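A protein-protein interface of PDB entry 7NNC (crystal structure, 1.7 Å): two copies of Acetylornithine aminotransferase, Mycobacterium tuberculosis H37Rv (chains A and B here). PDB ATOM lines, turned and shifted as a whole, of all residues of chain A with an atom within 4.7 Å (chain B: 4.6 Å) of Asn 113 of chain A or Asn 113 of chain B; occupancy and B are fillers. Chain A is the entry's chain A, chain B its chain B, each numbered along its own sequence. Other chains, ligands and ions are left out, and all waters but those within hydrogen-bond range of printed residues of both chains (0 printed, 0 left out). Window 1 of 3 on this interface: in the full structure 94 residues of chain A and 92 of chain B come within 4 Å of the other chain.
Of the printed residues of chain B, Pro 262 of chain A touches Asn 113 (3.6 Å) and Phe 285 (3.6 Å). Printed residues of chain A within 4 Å of Phe 285 of chain B: Asn 113, Pro 262 and Ile 263. Gly 286 of chain B touches none of the printed residues of chain A. The nearest printed residue of chain A that does not touch Asn 113 of chain B is Glu 117 of chain A (5.3 Å). The nearest printed residue of chain A that does not touch Ile 263 of chain B is Pro 262 of chain A (6.4 Å).
SG of Cys 112 of chain A sits at hydrogen-bond distance from O of Ser 114 of chain A (3.7 Å). The backbone NH (N) of Asn 113 of chain A sits at hydrogen-bond distance from the side-chain carboxylate (OE1) of Glu 117 of chain A. ND2 of Asn 113 of chain A is in hydrogen-bond range of OG of Ser 283 of chain A (3.2 Å). The side-chain sulfur (SG) of Cys 112 of chain B is in hydrogen-bond range of the backbone carbonyl oxygen (O) of Ser 114 of chain B (3.7 Å). The side-chain hydroxyl of Ser 283 of chain B is in hydrogen-bond range of the side-chain amide nitrogen of Asn 113 of chain B (3.2 Å). The side-chain hydroxyl of Ser 114 of chain B sits at hydrogen-bond distance from the backbone NH of Glu 117 of chain B.
OE2 of Glu 117 of chain B lies within hydrogen-bond range of OG of Ser 114 of chain A, 2.5 Å away. OE2 of Glu 117 of chain A lies within hydrogen-bond range of OG of Ser 114 of chain B, at 2.5 Å.
Asn 113 of chain A touches Pro 262 of chain B, and with the chains exchanged Pro 262 of chain A touches Asn 113 of chain B. Asn 113 of chain A touches Phe 285 of chain B, and with the chains exchanged Phe 285 of chain A touches Asn 113 of chain B. Glu 117 of chain A touches its own counterpart, Glu 117 of chain B. Ile 263 of chain A touches Phe 285 of chain B, and with the chains exchanged Phe 285 of chain A touches Ile 263 of chain B. Positions printed for both chains: 112, 113, 114, 117, 262, 263, 264, 283, 285 and 286. Of the 14 pairs that touch across the chains among the printed residues, 14 have their exchanged pair printed and touching as well.
Among the printed residues, merely in contact across the chains: Asn 113 of chain A with Phe 285 of chain B (3.2 Å), Phe 285 of chain A with Asn 113 of chain B (3.3 Å), Asn 113 of chain A with Asn 113 of chain B (3.5 Å), Phe 285 of chain A with Ile 263 of chain B (3.5 Å), Phe 285 of chain A with Pro 262 of chain B (3.6 Å), Pro 262 of chain A with Phe 285 of chain B (3.6 Å), Ile 263 of chain A with Phe 285 of chain B (3.6 Å), Pro 262 of chain A with Asn 113 of chain B (3.6 Å), Asn 113 of chain A with Ser 114 of chain B (3.6 Å), Ser 114 of chain A with Asn 113 of chain B (3.6 Å), Asn 113 of chain A with Pro 262 of chain B (3.6 Å) and Glu 117 of chain A with Glu 117 of chain B (3.7 Å).
Hydrophobic or aromatic side chains of chain A within 4 Å of the printed part of chain B: Pro 262 and Phe 285. Of the 10 printed residues of chain B, 6 touch a printed residue of chain A. Hydrophobic or aromatic side chains of chain B within 4 Å of the printed part of chain A: Pro 262 and Phe 285. Along chain B the printed residues that touch a printed residue of chain A span positions 113 to 285. Among the printed residues, no Asp or Glu carboxylate lies within 4 Å of a Lys or Arg side-chain nitrogen of the other chain.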
ATOM      1  N   CYS A 112       1.153  -1.720  19.258  1.00  0.00           N
ATOM      2  CA  CYS A 112       1.175  -1.188  20.614  1.00  0.00           C
ATOM      3  C   CYS A 112       0.011  -0.213  20.740  1.00  0.00           C
ATOM      4  O   CYS A 112      -0.951  -0.279  19.966  1.00  0.00           O
ATOM      5  CB  CYS A 112       2.555  -0.587  20.921  1.00  0.00           C
ATOM      6  SG  CYS A 112       3.039   0.643  19.735  1.00  0.00           S
ATOM      7  N   ASN A 113       0.081   0.700  21.712  1.00  0.00           N
ATOM      8  CA  ASN A 113      -1.096   1.496  22.059  1.00  0.00           C
ATOM      9  C   ASN A 113      -0.970   2.972  21.752  1.00  0.00           C
ATOM     10  O   ASN A 113      -1.970   3.683  21.853  1.00  0.00           O
ATOM     11  CB  ASN A 113      -1.400   1.380  23.555  1.00  0.00           C
ATOM     12  CG  ASN A 113      -1.655  -0.026  23.982  1.00  0.00           C
ATOM     13  OD1 ASN A 113      -2.623  -0.659  23.553  1.00  0.00           O
ATOM     14  ND2 ASN A 113      -0.732  -0.564  24.773  1.00  0.00           N
ATOM     15  N   SER A 114       0.216   3.460  21.415  1.00  0.00           N
ATOM     16  CA  SER A 114       0.426   4.899  21.369  1.00  0.00           C
ATOM     17  C   SER A 114       1.618   5.197  20.479  1.00  0.00           C
ATOM     18  O   SER A 114       2.392   4.306  20.115  1.00  0.00           O
ATOM     19  CB  SER A 114       0.670   5.453  22.776  1.00  0.00           C
ATOM     20  OG  SER A 114       1.924   4.960  23.261  1.00  0.00           O
ATOM     21  N   GLU A 117       4.782   4.573  22.492  1.00  0.00           N
ATOM     22  CA  GLU A 117       5.127   3.154  22.539  1.00  0.00           C
ATOM     23  C   GLU A 117       5.680   2.672  21.206  1.00  0.00           C
ATOM     24  O   GLU A 117       6.548   1.796  21.174  1.00  0.00           O
ATOM     25  CB  GLU A 117       3.903   2.323  22.933  1.00  0.00           C
ATOM     26  CG  GLU A 117       3.638   2.363  24.438  1.00  0.00           C
ATOM     27  CD  GLU A 117       2.558   1.375  24.890  1.00  0.00           C
ATOM     28  OE1 GLU A 117       1.819   0.839  24.043  1.00  0.00           O
ATOM     29  OE2 GLU A 117       2.465   1.115  26.108  1.00  0.00           O
ATOM     30  N   PRO A 262      -7.379   3.635  20.718  1.00  0.00           N
ATOM     31  CA  PRO A 262      -5.921   3.654  20.959  1.00  0.00           C
ATOM     32  C   PRO A 262      -5.224   2.484  20.283  1.00  0.00           C
ATOM     33  O   PRO A 262      -5.465   1.323  20.619  1.00  0.00           O
ATOM     34  CB  PRO A 262      -5.798   3.581  22.490  1.00  0.00           C
ATOM     35  CG  PRO A 262      -7.157   3.986  23.002  1.00  0.00           C
ATOM     36  CD  PRO A 262      -8.139   3.462  21.966  1.00  0.00           C
ATOM     37  N   ILE A 263      -4.329   2.802  19.350  1.00  0.00           N
ATOM     38  CA  ILE A 263      -3.516   1.793  18.684  1.00  0.00           C
ATOM     39  C   ILE A 263      -2.341   2.494  18.028  1.00  0.00           C
ATOM     40  O   ILE A 263      -2.476   3.603  17.497  1.00  0.00           O
ATOM     41  CB  ILE A 263      -4.335   0.963  17.666  1.00  0.00           C
ATOM     42  CG1 ILE A 263      -3.463  -0.083  16.988  1.00  0.00           C
ATOM     43  CG2 ILE A 263      -4.997   1.849  16.607  1.00  0.00           C
ATOM     44  CD1 ILE A 263      -4.260  -1.226  16.355  1.00  0.00           C
ATOM     45  N   GLY A 264      -1.181   1.838  18.091  1.00  0.00           N
ATOM     46  CA  GLY A 264      -0.005   2.282  17.375  1.00  0.00           C
ATOM     47  C   GLY A 264       0.668   1.089  16.730  1.00  0.00           C
ATOM     48  O   GLY A 264       0.340  -0.068  17.029  1.00  0.00           O
ATOM     49  N   SER A 283       3.612  -5.943  24.419  1.00  0.00           N
ATOM     50  CA  SER A 283       2.657  -4.996  24.997  1.00  0.00           C
ATOM     51  C   SER A 283       1.359  -5.763  25.193  1.00  0.00           C
ATOM     52  O   SER A 283       0.854  -6.339  24.228  1.00  0.00           O
ATOM     53  CB  SER A 283       2.439  -3.792  24.074  1.00  0.00           C
ATOM     54  OG  SER A 283       1.610  -2.810  24.699  1.00  0.00           O
ATOM     55  N   PHE A 285      -1.883  -5.136  25.559  1.00  0.00           N
ATOM     56  CA  PHE A 285      -3.012  -4.788  24.698  1.00  0.00           C
ATOM     57  C   PHE A 285      -2.667  -4.738  23.209  1.00  0.00           C
ATOM     58  O   PHE A 285      -3.570  -4.481  22.393  1.00  0.00           O
ATOM     59  CB  PHE A 285      -3.585  -3.404  25.056  1.00  0.00           C
ATOM     60  CG  PHE A 285      -4.073  -3.232  26.471  1.00  0.00           C
ATOM     61  CD1 PHE A 285      -4.954  -4.145  27.072  1.00  0.00           C
ATOM     62  CD2 PHE A 285      -3.708  -2.098  27.186  1.00  0.00           C
ATOM     63  CE1 PHE A 285      -5.432  -3.921  28.357  1.00  0.00           C
ATOM     64  CE2 PHE A 285      -4.191  -1.858  28.453  1.00  0.00           C
ATOM     65  CZ  PHE A 285      -5.046  -2.771  29.057  1.00  0.00           C
ATOM     66  N   GLY A 286      -1.402  -4.914  22.833  1.00  0.00           N
ATOM     67  CA  GLY A 286      -0.995  -4.687  21.447  1.00  0.00           C
ATOM     68  C   GLY A 286      -1.719  -5.600  20.477  1.00  0.00           C
ATOM     69  O   GLY A 286      -1.803  -6.810  20.707  1.00  0.00           O
ATOM     70  N   CYS B 112      -3.421   6.953  30.797  1.00  0.00           N
ATOM     71  CA  CYS B 112      -2.571   6.577  29.680  1.00  0.00           C
ATOM     72  C   CYS B 112      -3.133   5.283  29.102  1.00  0.00           C
ATOM     73  O   CYS B 112      -4.305   4.959  29.312  1.00  0.00           O
ATOM     74  CB  CYS B 112      -1.110   6.478  30.142  1.00  0.00           C
ATOM     75  SG  CYS B 112      -0.884   5.346  31.547  1.00  0.00           S
ATOM     76  N   ASN B 113      -2.305   4.533  28.374  1.00  0.00           N
ATOM     77  CA  ASN B 113      -2.833   3.431  27.583  1.00  0.00           C
ATOM     78  C   ASN B 113      -2.385   2.055  28.022  1.00  0.00           C
ATOM     79  O   ASN B 113      -2.863   1.071  27.448  1.00  0.00           O
ATOM     80  CB  ASN B 113      -2.423   3.574  26.120  1.00  0.00           C
ATOM     81  CG  ASN B 113      -2.862   4.865  25.533  1.00  0.00           C
ATOM     82  OD1 ASN B 113      -4.045   5.061  25.283  1.00  0.00           O
ATOM     83  ND2 ASN B 113      -1.910   5.774  25.312  1.00  0.00           N
ATOM     84  N   SER B 114      -1.447   1.948  28.949  1.00  0.00           N
ATOM     85  CA  SER B 114      -0.867   0.635  29.196  1.00  0.00           C
ATOM     86  C   SER B 114      -0.243   0.654  30.577  1.00  0.00           C
ATOM     87  O   SER B 114      -0.081   1.712  31.192  1.00  0.00           O
ATOM     88  CB  SER B 114       0.207   0.291  28.160  1.00  0.00           C
ATOM     89  OG  SER B 114       1.277   1.245  28.257  1.00  0.00           O
ATOM     90  N   GLU B 117       3.128   2.429  30.286  1.00  0.00           N
ATOM     91  CA  GLU B 117       3.031   3.883  30.297  1.00  0.00           C
ATOM     92  C   GLU B 117       2.669   4.387  31.685  1.00  0.00           C
ATOM     93  O   GLU B 117       3.085   5.489  32.066  1.00  0.00           O
ATOM     94  CB  GLU B 117       1.982   4.380  29.300  1.00  0.00           C
ATOM     95  CG  GLU B 117       2.450   4.331  27.854  1.00  0.00           C
ATOM     96  CD  GLU B 117       1.474   5.009  26.895  1.00  0.00           C
ATOM     97  OE1 GLU B 117       0.273   5.107  27.215  1.00  0.00           O
ATOM     98  OE2 GLU B 117       1.891   5.335  25.761  1.00  0.00           O
ATOM     99  N   PRO B 262      -7.989  -0.682  25.930  1.00  0.00           N
ATOM    100  CA  PRO B 262      -6.658  -0.270  26.420  1.00  0.00           C
ATOM    101  C   PRO B 262      -6.766   1.004  27.245  1.00  0.00           C
ATOM    102  O   PRO B 262      -7.143   2.056  26.729  1.00  0.00           O
ATOM    103  CB  PRO B 262      -5.840  -0.041  25.139  1.00  0.00           C
ATOM    104  CG  PRO B 262      -6.649  -0.618  24.019  1.00  0.00           C
ATOM    105  CD  PRO B 262      -8.086  -0.720  24.461  1.00  0.00           C
ATOM    106  N   ILE B 263      -6.409   0.910  28.523  1.00  0.00           N
ATOM    107  CA  ILE B 263      -6.369   2.084  29.388  1.00  0.00           C
ATOM    108  C   ILE B 263      -5.496   1.764  30.591  1.00  0.00           C
ATOM    109  O   ILE B 263      -5.467   0.628  31.071  1.00  0.00           O
ATOM    110  CB  ILE B 263      -7.791   2.538  29.802  1.00  0.00           C
ATOM    111  CG1 ILE B 263      -7.733   3.766  30.736  1.00  0.00           C
ATOM    112  CG2 ILE B 263      -8.604   1.391  30.415  1.00  0.00           C
ATOM    113  CD1 ILE B 263      -9.087   4.510  30.803  1.00  0.00           C
ATOM    114  N   GLY B 264      -4.767   2.784  31.055  1.00  0.00           N
ATOM    115  CA  GLY B 264      -3.970   2.675  32.255  1.00  0.00           C
ATOM    116  C   GLY B 264      -4.074   3.958  33.055  1.00  0.00           C
ATOM    117  O   GLY B 264      -4.583   4.965  32.569  1.00  0.00           O
ATOM    118  N   SER B 283      -0.264  12.209  27.119  1.00  0.00           N
ATOM    119  CA  SER B 283      -0.472  11.059  26.236  1.00  0.00           C
ATOM    120  C   SER B 283      -1.693  11.371  25.385  1.00  0.00           C
ATOM    121  O   SER B 283      -2.757  11.658  25.942  1.00  0.00           O
ATOM    122  CB  SER B 283      -0.700   9.782  27.043  1.00  0.00           C
ATOM    123  OG  SER B 283      -0.737   8.638  26.194  1.00  0.00           O
ATOM    124  N   PHE B 285      -3.950   9.716  23.600  1.00  0.00           N
ATOM    125  CA  PHE B 285      -5.178   8.950  23.823  1.00  0.00           C
ATOM    126  C   PHE B 285      -5.605   8.899  25.288  1.00  0.00           C
ATOM    127  O   PHE B 285      -6.670   8.338  25.583  1.00  0.00           O
ATOM    128  CB  PHE B 285      -5.001   7.495  23.375  1.00  0.00           C
ATOM    129  CG  PHE B 285      -4.710   7.297  21.902  1.00  0.00           C
ATOM    130  CD1 PHE B 285      -5.424   7.970  20.910  1.00  0.00           C
ATOM    131  CD2 PHE B 285      -3.699   6.409  21.519  1.00  0.00           C
ATOM    132  CE1 PHE B 285      -5.154   7.740  19.565  1.00  0.00           C
ATOM    133  CE2 PHE B 285      -3.425   6.168  20.186  1.00  0.00           C
ATOM    134  CZ  PHE B 285      -4.153   6.837  19.199  1.00  0.00           C
ATOM    135  N   GLY B 286      -4.792   9.421  26.209  1.00  0.00           N
ATOM    136  CA  GLY B 286      -5.053   9.228  27.627  1.00  0.00           C
ATOM    137  C   GLY B 286      -6.392   9.785  28.077  1.00  0.00           C
ATOM    138  O   GLY B 286      -6.731  10.938  27.780  1.00  0.00           O
